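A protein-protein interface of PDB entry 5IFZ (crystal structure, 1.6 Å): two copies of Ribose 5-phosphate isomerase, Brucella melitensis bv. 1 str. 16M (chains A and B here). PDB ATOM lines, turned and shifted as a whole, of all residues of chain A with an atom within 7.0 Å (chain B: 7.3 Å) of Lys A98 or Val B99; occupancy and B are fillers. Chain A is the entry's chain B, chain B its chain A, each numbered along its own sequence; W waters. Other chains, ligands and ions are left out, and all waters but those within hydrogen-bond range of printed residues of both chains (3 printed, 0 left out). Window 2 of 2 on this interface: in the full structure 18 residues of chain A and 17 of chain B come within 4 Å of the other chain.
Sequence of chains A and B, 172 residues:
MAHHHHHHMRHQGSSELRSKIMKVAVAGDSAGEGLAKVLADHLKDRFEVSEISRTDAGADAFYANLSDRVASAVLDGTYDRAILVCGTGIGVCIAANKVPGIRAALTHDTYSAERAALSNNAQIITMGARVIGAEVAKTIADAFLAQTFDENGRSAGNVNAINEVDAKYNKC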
ATOM      1  N   VAL A  92       4.853  16.915   3.684  1.00  0.00           N
ATOM      2  CA  VAL A  92       6.239  16.460   3.601  1.00  0.00           C
ATOM      3  C   VAL A  92       6.386  15.397   2.530  1.00  0.00           C
ATOM      4  O   VAL A  92       7.457  15.260   1.926  1.00  0.00           O
ATOM      5  CB  VAL A  92       6.747  15.935   4.960  1.00  0.00           C
ATOM      6  CG1 VAL A  92       7.258  17.070   5.796  1.00  0.00           C
ATOM      7  CG2 VAL A  92       5.649  15.154   5.687  1.00  0.00           C
ATOM      8  N   CYS A  93       5.342  14.602   2.306  1.00  0.00           N
ATOM      9  CA  CYS A  93       5.405  13.598   1.256  1.00  0.00           C
ATOM     10  C   CYS A  93       5.478  14.256  -0.116  1.00  0.00           C
ATOM     11  O   CYS A  93       6.313  13.880  -0.945  1.00  0.00           O
ATOM     12  CB  CYS A  93       4.205  12.653   1.354  1.00  0.00           C
ATOM     13  SG  CYS A  93       4.183  11.345   0.106  1.00  0.00           S
ATOM     14  N   ILE A  94       4.606  15.240  -0.370  1.00  0.00           N
ATOM     15  CA  ILE A  94       4.651  15.986  -1.625  1.00  0.00           C
ATOM     16  C   ILE A  94       6.035  16.588  -1.821  1.00  0.00           C
ATOM     17  O   ILE A  94       6.670  16.411  -2.867  1.00  0.00           O
ATOM     18  CB  ILE A  94       3.563  17.076  -1.641  1.00  0.00           C
ATOM     19  CG1 ILE A  94       2.156  16.474  -1.646  1.00  0.00           C
ATOM     20  CG2 ILE A  94       3.762  18.003  -2.838  1.00  0.00           C
ATOM     21  CD1 ILE A  94       1.065  17.503  -1.337  1.00  0.00           C
ATOM     22  N   ALA A  95       6.528  17.292  -0.800  1.00  0.00           N
ATOM     23  CA  ALA A  95       7.774  18.038  -0.936  1.00  0.00           C
ATOM     24  C   ALA A  95       8.967  17.112  -1.142  1.00  0.00           C
ATOM     25  O   ALA A  95       9.868  17.423  -1.933  1.00  0.00           O
ATOM     26  CB  ALA A  95       7.990  18.923   0.292  1.00  0.00           C
ATOM     27  N   ALA A  96       8.994  15.971  -0.434  1.00  0.00           N
ATOM     28  CA  ALA A  96      10.116  15.049  -0.581  1.00  0.00           C
ATOM     29  C   ALA A  96      10.119  14.410  -1.963  1.00  0.00           C
ATOM     30  O   ALA A  96      11.180  14.268  -2.588  1.00  0.00           O
ATOM     31  CB  ALA A  96      10.074  13.975   0.515  1.00  0.00           C
ATOM     32  N   ASN A  97       8.937  14.063  -2.480  1.00  0.00           N
ATOM     33  CA  ASN A  97       8.863  13.456  -3.803  1.00  0.00           C
ATOM     34  C   ASN A  97       9.249  14.421  -4.926  1.00  0.00           C
ATOM     35  O   ASN A  97       9.630  13.965  -6.015  1.00  0.00           O
ATOM     36  CB  ASN A  97       7.466  12.881  -4.018  1.00  0.00           C
ATOM     37  CG  ASN A  97       7.332  11.498  -3.432  1.00  0.00           C
ATOM     38  OD1 ASN A  97       8.176  10.643  -3.688  1.00  0.00           O
ATOM     39  ND2 ASN A  97       6.279  11.266  -2.643  1.00  0.00           N
ATOM     40  N   LYS A  98       9.188  15.737  -4.685  1.00  0.00           N
ATOM     41  CA  LYS A  98       9.641  16.732  -5.653  1.00  0.00           C
ATOM     42  C   LYS A  98      11.158  16.834  -5.741  1.00  0.00           C
ATOM     43  O   LYS A  98      11.662  17.536  -6.627  1.00  0.00           O
ATOM     44  CB  LYS A  98       9.082  18.112  -5.305  1.00  0.00           C
ATOM     45  CG  LYS A  98       7.583  18.205  -5.199  1.00  0.00           C
ATOM     46  CD  LYS A  98       6.922  18.134  -6.534  1.00  0.00           C
ATOM     47  CE  LYS A  98       5.457  18.529  -6.447  1.00  0.00           C
ATOM     48  NZ  LYS A  98       4.868  18.497  -7.809  1.00  0.00           N
ATOM     49  N   VAL A  99      11.892  16.198  -4.830  1.00  0.00           N
ATOM     50  CA  VAL A  99      13.352  16.148  -4.916  1.00  0.00           C
ATOM     51  C   VAL A  99      13.722  15.029  -5.882  1.00  0.00           C
ATOM     52  O   VAL A  99      13.371  13.864  -5.632  1.00  0.00           O
ATOM     53  CB  VAL A  99      14.002  15.921  -3.542  1.00  0.00           C
ATOM     54  CG1 VAL A  99      15.524  15.938  -3.668  1.00  0.00           C
ATOM     55  CG2 VAL A  99      13.524  16.963  -2.537  1.00  0.00           C
ATOM     56  N   PRO A 100      14.400  15.324  -6.990  1.00  0.00           N
ATOM     57  CA  PRO A 100      14.757  14.259  -7.935  1.00  0.00           C
ATOM     58  C   PRO A 100      15.573  13.174  -7.249  1.00  0.00           C
ATOM     59  O   PRO A 100      16.550  13.454  -6.552  1.00  0.00           O
ATOM     60  CB  PRO A 100      15.572  14.994  -9.002  1.00  0.00           C
ATOM     61  CG  PRO A 100      15.096  16.397  -8.917  1.00  0.00           C
ATOM     62  CD  PRO A 100      14.814  16.650  -7.476  1.00  0.00           C
ATOM     63  N   GLY A 101      15.144  11.927  -7.431  1.00  0.00           N
ATOM     64  CA  GLY A 101      15.818  10.790  -6.851  1.00  0.00           C
ATOM     65  C   GLY A 101      15.234  10.311  -5.540  1.00  0.00           C
ATOM     66  O   GLY A 101      15.596   9.219  -5.084  1.00  0.00           O
ATOM     67  N   ILE A 102      14.347  11.087  -4.922  1.00  0.00           N
ATOM     68  CA  ILE A 102      13.738  10.732  -3.642  1.00  0.00           C
ATOM     69  C   ILE A 102      12.380  10.093  -3.896  1.00  0.00           C
ATOM     70  O   ILE A 102      11.562  10.627  -4.655  1.00  0.00           O
ATOM     71  CB  ILE A 102      13.591  11.964  -2.734  1.00  0.00           C
ATOM     72  CG1 ILE A 102      14.961  12.460  -2.274  1.00  0.00           C
ATOM     73  CG2 ILE A 102      12.692  11.634  -1.543  1.00  0.00           C
ATOM     74  CD1 ILE A 102      15.710  11.461  -1.412  1.00  0.00           C
ATOM     75  N   SER B  67      -0.746   7.235 -13.615  1.00  0.00           N
ATOM     76  CA  SER B  67      -0.610   8.444 -12.809  1.00  0.00           C
ATOM     77  C   SER B  67      -0.179   9.626 -13.663  1.00  0.00           C
ATOM     78  O   SER B  67      -0.748  10.718 -13.567  1.00  0.00           O
ATOM     79  CB  SER B  67       0.406   8.219 -11.692  1.00  0.00           C
ATOM     80  OG  SER B  67       0.127   7.033 -10.988  1.00  0.00           O
ATOM     81  N   ASP B  68       0.845   9.421 -14.497  1.00  0.00           N
ATOM     82  CA  ASP B  68       1.369  10.509 -15.322  1.00  0.00           C
ATOM     83  C   ASP B  68       0.323  11.016 -16.308  1.00  0.00           C
ATOM     84  O   ASP B  68       0.151  12.233 -16.476  1.00  0.00           O
ATOM     85  CB  ASP B  68       2.622  10.052 -16.072  1.00  0.00           C
ATOM     86  CG  ASP B  68       3.848   9.982 -15.182  1.00  0.00           C
ATOM     87  OD1 ASP B  68       3.820  10.537 -14.062  1.00  0.00           O
ATOM     88  OD2 ASP B  68       4.845   9.367 -15.608  1.00  0.00           O
ATOM     89  N   ARG B  69      -0.379  10.101 -16.983  1.00  0.00           N
ATOM     90  CA  ARG B  69      -1.375  10.523 -17.970  1.00  0.00           C
ATOM     91  C   ARG B  69      -2.507  11.308 -17.316  1.00  0.00           C
ATOM     92  O   ARG B  69      -2.930  12.354 -17.823  1.00  0.00           O
ATOM     93  CB  ARG B  69      -1.924   9.307 -18.720  1.00  0.00           C
ATOM     94  N   VAL B  70      -3.014  10.818 -16.185  1.00  0.00           N
ATOM     95  CA  VAL B  70      -4.106  11.505 -15.505  1.00  0.00           C
ATOM     96  C   VAL B  70      -3.620  12.823 -14.917  1.00  0.00           C
ATOM     97  O   VAL B  70      -4.300  13.854 -15.015  1.00  0.00           O
ATOM     98  CB  VAL B  70      -4.720  10.581 -14.434  1.00  0.00           C
ATOM     99  CG1 VAL B  70      -5.778  11.327 -13.643  1.00  0.00           C
ATOM    100  CG2 VAL B  70      -5.322   9.361 -15.093  1.00  0.00           C
ATOM    101  N   ALA B  71      -2.435  12.817 -14.298  1.00  0.00           N
ATOM    102  CA  ALA B  71      -1.890  14.050 -13.733  1.00  0.00           C
ATOM    103  C   ALA B  71      -1.697  15.106 -14.812  1.00  0.00           C
ATOM    104  O   ALA B  71      -1.968  16.291 -14.581  1.00  0.00           O
ATOM    105  CB  ALA B  71      -0.568  13.774 -13.017  1.00  0.00           C
ATOM    106  N   SER B  72      -1.238  14.694 -15.995  1.00  0.00           N
ATOM    107  CA  SER B  72      -1.052  15.653 -17.076  1.00  0.00           C
ATOM    108  C   SER B  72      -2.385  16.212 -17.542  1.00  0.00           C
ATOM    109  O   SER B  72      -2.472  17.395 -17.904  1.00  0.00           O
ATOM    110  CB  SER B  72      -0.311  14.999 -18.240  1.00  0.00           C
ATOM    111  OG  SER B  72       0.975  14.576 -17.840  1.00  0.00           O
ATOM    112  N   LEU B  75      -3.387  18.768 -15.109  1.00  0.00           N
ATOM    113  CA  LEU B  75      -2.557  19.953 -15.284  1.00  0.00           C
ATOM    114  C   LEU B  75      -3.033  20.807 -16.454  1.00  0.00           C
ATOM    115  O   LEU B  75      -3.052  22.041 -16.363  1.00  0.00           O
ATOM    116  CB  LEU B  75      -1.104  19.534 -15.488  1.00  0.00           C
ATOM    117  CG  LEU B  75      -0.023  20.538 -15.127  1.00  0.00           C
ATOM    118  CD1 LEU B  75      -0.189  20.986 -13.686  1.00  0.00           C
ATOM    119  CD2 LEU B  75       1.339  19.904 -15.347  1.00  0.00           C
ATOM    120  N   CYS B  93       0.867   8.092  -5.821  1.00  0.00           N
ATOM    121  CA  CYS B  93       1.176   9.350  -5.151  1.00  0.00           C
ATOM    122  C   CYS B  93       2.584   9.819  -5.497  1.00  0.00           C
ATOM    123  O   CYS B  93       2.790  10.985  -5.858  1.00  0.00           O
ATOM    124  CB  CYS B  93       1.005   9.180  -3.639  1.00  0.00           C
ATOM    125  SG  CYS B  93       1.367  10.681  -2.697  1.00  0.00           S
ATOM    126  N   ILE B  94       3.564   8.911  -5.434  1.00  0.00           N
ATOM    127  CA  ILE B  94       4.936   9.255  -5.819  1.00  0.00           C
ATOM    128  C   ILE B  94       4.978   9.760  -7.256  1.00  0.00           C
ATOM    129  O   ILE B  94       5.555  10.813  -7.553  1.00  0.00           O
ATOM    130  CB  ILE B  94       5.864   8.041  -5.640  1.00  0.00           C
ATOM    131  CG1 ILE B  94       5.986   7.670  -4.162  1.00  0.00           C
ATOM    132  CG2 ILE B  94       7.237   8.329  -6.256  1.00  0.00           C
ATOM    133  CD1 ILE B  94       6.821   6.413  -3.919  1.00  0.00           C
ATOM    134  N   ALA B  95       4.374   9.001  -8.171  1.00  0.00           N
ATOM    135  CA  ALA B  95       4.460   9.339  -9.585  1.00  0.00           C
ATOM    136  C   ALA B  95       3.784  10.668  -9.878  1.00  0.00           C
ATOM    137  O   ALA B  95       4.299  11.468 -10.666  1.00  0.00           O
ATOM    138  CB  ALA B  95       3.833   8.226 -10.421  1.00  0.00           C
ATOM    139  N   ALA B  96       2.616  10.909  -9.275  1.00  0.00           N
ATOM    140  CA  ALA B  96       1.894  12.144  -9.586  1.00  0.00           C
ATOM    141  C   ALA B  96       2.641  13.366  -9.069  1.00  0.00           C
ATOM    142  O   ALA B  96       2.669  14.409  -9.730  1.00  0.00           O
ATOM    143  CB  ALA B  96       0.483  12.100  -9.008  1.00  0.00           C
ATOM    144  N   ASN B  97       3.246  13.265  -7.884  1.00  0.00           N
ATOM    145  CA  ASN B  97       3.999  14.402  -7.366  1.00  0.00           C
ATOM    146  C   ASN B  97       5.253  14.690  -8.175  1.00  0.00           C
ATOM    147  O   ASN B  97       5.777  15.810  -8.116  1.00  0.00           O
ATOM    148  CB  ASN B  97       4.348  14.163  -5.899  1.00  0.00           C
ATOM    149  CG  ASN B  97       3.193  14.483  -4.987  1.00  0.00           C
ATOM    150  OD1 ASN B  97       2.621  15.565  -5.063  1.00  0.00           O
ATOM    151  ND2 ASN B  97       2.822  13.535  -4.135  1.00  0.00           N
ATOM    152  N   LYS B  98       5.726  13.738  -8.966  1.00  0.00           N
ATOM    153  CA  LYS B  98       6.878  13.998  -9.813  1.00  0.00           C
ATOM    154  C   LYS B  98       6.490  14.628 -11.148  1.00  0.00           C
ATOM    155  O   LYS B  98       7.357  14.829 -12.007  1.00  0.00           O
ATOM    156  CB  LYS B  98       7.685  12.715 -10.001  1.00  0.00           C
ATOM    157  CG  LYS B  98       8.427  12.374  -8.715  1.00  0.00           C
ATOM    158  CD  LYS B  98       9.314  11.167  -8.829  1.00  0.00           C
ATOM    159  CE  LYS B  98       9.947  10.862  -7.477  1.00  0.00           C
ATOM    160  NZ  LYS B  98      10.933  11.914  -7.074  1.00  0.00           N
ATOM    161  N   VAL B  99       5.218  14.964 -11.331  1.00  0.00           N
ATOM    162  CA  VAL B  99       4.780  15.800 -12.444  1.00  0.00           C
ATOM    163  C   VAL B  99       4.837  17.250 -11.979  1.00  0.00           C
ATOM    164  O   VAL B  99       4.118  17.608 -11.029  1.00  0.00           O
ATOM    165  CB  VAL B  99       3.367  15.436 -12.911  1.00  0.00           C
ATOM    166  CG1 VAL B  99       2.924  16.376 -14.022  1.00  0.00           C
ATOM    167  CG2 VAL B  99       3.316  13.970 -13.374  1.00  0.00           C
ATOM    168  N   PRO B 100       5.661  18.098 -12.591  1.00  0.00           N
ATOM    169  CA  PRO B 100       5.767  19.485 -12.124  1.00  0.00           C
ATOM    170  C   PRO B 100       4.416  20.185 -12.164  1.00  0.00           C
ATOM    171  O   PRO B 100       3.710  20.155 -13.175  1.00  0.00           O
ATOM    172  CB  PRO B 100       6.768  20.114 -13.104  1.00  0.00           C
ATOM    173  CG  PRO B 100       7.577  18.955 -13.593  1.00  0.00           C
ATOM    174  CD  PRO B 100       6.603  17.811 -13.686  1.00  0.00           C
ATOM    175  N   GLY B 101       4.054  20.802 -11.041  1.00  0.00           N
ATOM    176  CA  GLY B 101       2.809  21.526 -10.931  1.00  0.00           C
ATOM    177  C   GLY B 101       1.665  20.737 -10.336  1.00  0.00           C
ATOM    178  O   GLY B 101       0.593  21.309 -10.108  1.00  0.00           O
ATOM    179  N   ILE B 102       1.852  19.443 -10.096  1.00  0.00           N
ATOM    180  CA  ILE B 102       0.819  18.577  -9.537  1.00  0.00           C
ATOM    181  C   ILE B 102       1.142  18.304  -8.076  1.00  0.00           C
ATOM    182  O   ILE B 102       2.292  18.004  -7.730  1.00  0.00           O
ATOM    183  CB  ILE B 102       0.709  17.263 -10.331  1.00  0.00           C
ATOM    184  CG1 ILE B 102       0.041  17.512 -11.678  1.00  0.00           C
ATOM    185  CG2 ILE B 102      -0.056  16.192  -9.541  1.00  0.00           C
ATOM    186  CD1 ILE B 102      -1.357  18.078 -11.571  1.00  0.00           C
ATOM    187  N   ARG B 103       0.132  18.426  -7.218  1.00  0.00           N
ATOM    188  CA  ARG B 103       0.226  18.030  -5.814  1.00  0.00           C
ATOM    189  C   ARG B 103      -0.743  16.882  -5.574  1.00  0.00           C
ATOM    190  O   ARG B 103      -1.948  17.014  -5.828  1.00  0.00           O
ATOM    191  CB  ARG B 103      -0.070  19.220  -4.893  1.00  0.00           C
ATOM    192  CG  ARG B 103       0.958  20.348  -5.035  1.00  0.00           C
ATOM    193  CD  ARG B 103       0.503  21.684  -4.427  1.00  0.00           C
ATOM    194  NE  ARG B 103      -0.788  22.134  -4.945  1.00  0.00           N
ATOM    195  CZ  ARG B 103      -0.969  22.801  -6.083  1.00  0.00           C
ATOM    196  NH1 ARG B 103       0.062  23.128  -6.855  1.00  0.00           N
ATOM    197  NH2 ARG B 103      -2.197  23.148  -6.449  1.00  0.00           N
ATOM    198  N   ALA B 104      -0.214  15.751  -5.106  1.00  0.00           N
ATOM    199  CA  ALA B 104      -1.011  14.553  -4.873  1.00  0.00           C
ATOM    200  C   ALA B 104      -0.896  14.112  -3.417  1.00  0.00           C
ATOM    201  O   ALA B 104       0.196  14.097  -2.839  1.00  0.00           O
ATOM    202  CB  ALA B 104      -0.578  13.406  -5.802  1.00  0.00           C
ATOM    203  N   GLN B 123      -4.499  18.727  -6.219  1.00  0.00           N
ATOM    204  CA  GLN B 123      -5.457  18.459  -7.276  1.00  0.00           C
ATOM    205  C   GLN B 123      -5.834  16.992  -7.349  1.00  0.00           C
ATOM    206  O   GLN B 123      -6.854  16.660  -7.961  1.00  0.00           O
ATOM    207  CB  GLN B 123      -4.912  18.894  -8.641  1.00  0.00           C
ATOM    208  CG  GLN B 123      -4.391  20.315  -8.705  1.00  0.00           C
ATOM    209  CD  GLN B 123      -2.882  20.357  -8.648  1.00  0.00           C
ATOM    210  OE1 GLN B 123      -2.266  19.583  -7.915  1.00  0.00           O
ATOM    211  NE2 GLN B 123      -2.278  21.234  -9.436  1.00  0.00           N
ATOM    212  N   ILE B 124      -5.024  16.112  -6.761  1.00  0.00           N
ATOM    213  CA  ILE B 124      -5.202  14.670  -6.870  1.00  0.00           C
ATOM    214  C   ILE B 124      -5.133  14.063  -5.478  1.00  0.00           C
ATOM    215  O   ILE B 124      -4.262  14.424  -4.680  1.00  0.00           O
ATOM    216  CB  ILE B 124      -4.120  14.052  -7.779  1.00  0.00           C
ATOM    217  CG1 ILE B 124      -4.259  14.590  -9.211  1.00  0.00           C
ATOM    218  CG2 ILE B 124      -4.172  12.523  -7.732  1.00  0.00           C
ATOM    219  CD1 ILE B 124      -3.191  14.085 -10.177  1.00  0.00           C
HETATM  220  O   HOH W   1       5.920  21.089  -8.816  1.00  0.00           O
HETATM  221  O   HOH W   2       1.478  13.340  -0.301  1.00  0.00           O
HETATM  222  O   HOH W   3       3.606   8.192  -1.603  1.00  0.00           O
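Printed residues of chain B that touch a printed residue of chain A: Ile B94, Asn B97, Lys B98, Val B99, Ile B102 and Ala B104. Hydrophobic or aromatic side chains of chain B that line the printed part of chain A: Ile B94. Of the 11 printed residues of chain A, 5 touch a printed residue of chain B. Among the printed residues, 10 pairs touch across the chains. Among the printed residues, no Asp or Glu carboxylate lies within 4 Å of a Lys or Arg side-chain nitrogen of the other chain.
The side-chain amino group of Lys A98 sits at hydrogen-bond distance from the backbone carbonyl oxygen of Asn B97, 2.9 Å away. O of Asn A97 lies within hydrogen-bond range of NZ of Lys B98, 2.7 Å away. The side-chain amino group (NZ) of Lys B98 is in hydrogen-bond range of the backbone carbonyl oxygen (O) of Val A99 (3.4 Å). O of Ile A102 sits at hydrogen-bond distance from NZ of Lys B98 (2.8 Å). The backbone carbonyl oxygen (O) of Val B99 is in hydrogen-bond range of the side-chain amino group (NZ) of Lys A98 (3.4 Å). The side-chain amino group (NZ) of Lys A98 is in hydrogen-bond range of the backbone carbonyl oxygen (O) of Ile B102, 2.6 Å away.
Ile A94 touches Asn B97, and with the chains exchanged Asn A97 touches Ile B94. Asn B97 touches its own counterpart, Asn A97. Asn A97 touches Lys B98, and with the chains exchanged Lys A98 touches Asn B97. Lys A98 touches Val B99, and with the chains exchanged Val A99 touches Lys B98. 10 positions are printed for both chains.
Among the printed residues, pairs that only touch across the chains: Ile A94 with Ala B104 (3.3 Å), Ile A94 with Asn B97 (3.5 Å), Asn A97 with Ile B94 (3.6 Å) and Asn A97 with Asn B97 (3.9 Å).
Water W1 bridges N of Gly B101 (2.9 Å) and NZ of Lys A98 (3.0 Å). Water W2 lies within hydrogen-bond range of O of Ala B104 (2.9 Å), SG of Cys A93 (3.4 Å) and SG of Cys B93 (3.6 Å). Water W3 bridges the side-chain sulfur of Cys B93 and the side-chain sulfur of Cys A93.
The backbone carbonyl oxygen of Cys B93 is in hydrogen-bond range of the side-chain amide nitrogen of Asn B97, at 3.1 Å. The side-chain sulfur (SG) of Cys B93 is in hydrogen-bond range of the backbone carbonyl oxygen (O) of Ala B104, at 3.6 Å. N of Ala B104 sits at hydrogen-bond distance from OD1 of Asn B97, 2.8 Å away. The side-chain amide nitrogen (ND2) of Asn A97 is in hydrogen-bond range of the backbone carbonyl oxygen (O) of Cys A93 (3.1 Å).
Lys A98 touches just these residues of chain B: Asn B97, Val B99 and Ile B102. Printed residues of chain A within 4 Å of Val B99: Lys A98 (3.4 Å). Of the printed residues of chain B, Ile A94 touches Asn B97 (3.5 Å) and Ala B104 (3.3 Å). Printed residues of chain A within 4 Å of Ile B94: Asn A97 (3.6 Å). Printed residues of chain B within 4 Å of Asn A97: Ile B94 (3.6 Å), Asn B97 (3.9 Å) and Lys B98 (2.7 Å). Asp B68 touches none of the printed residues of chain A. The nearest residue of chain B that does not touch Lys A98 is Gly B101 (4.1 Å). The nearest printed residue of chain A that does not touch Ile B94 is Ile A102 (5.2 Å).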
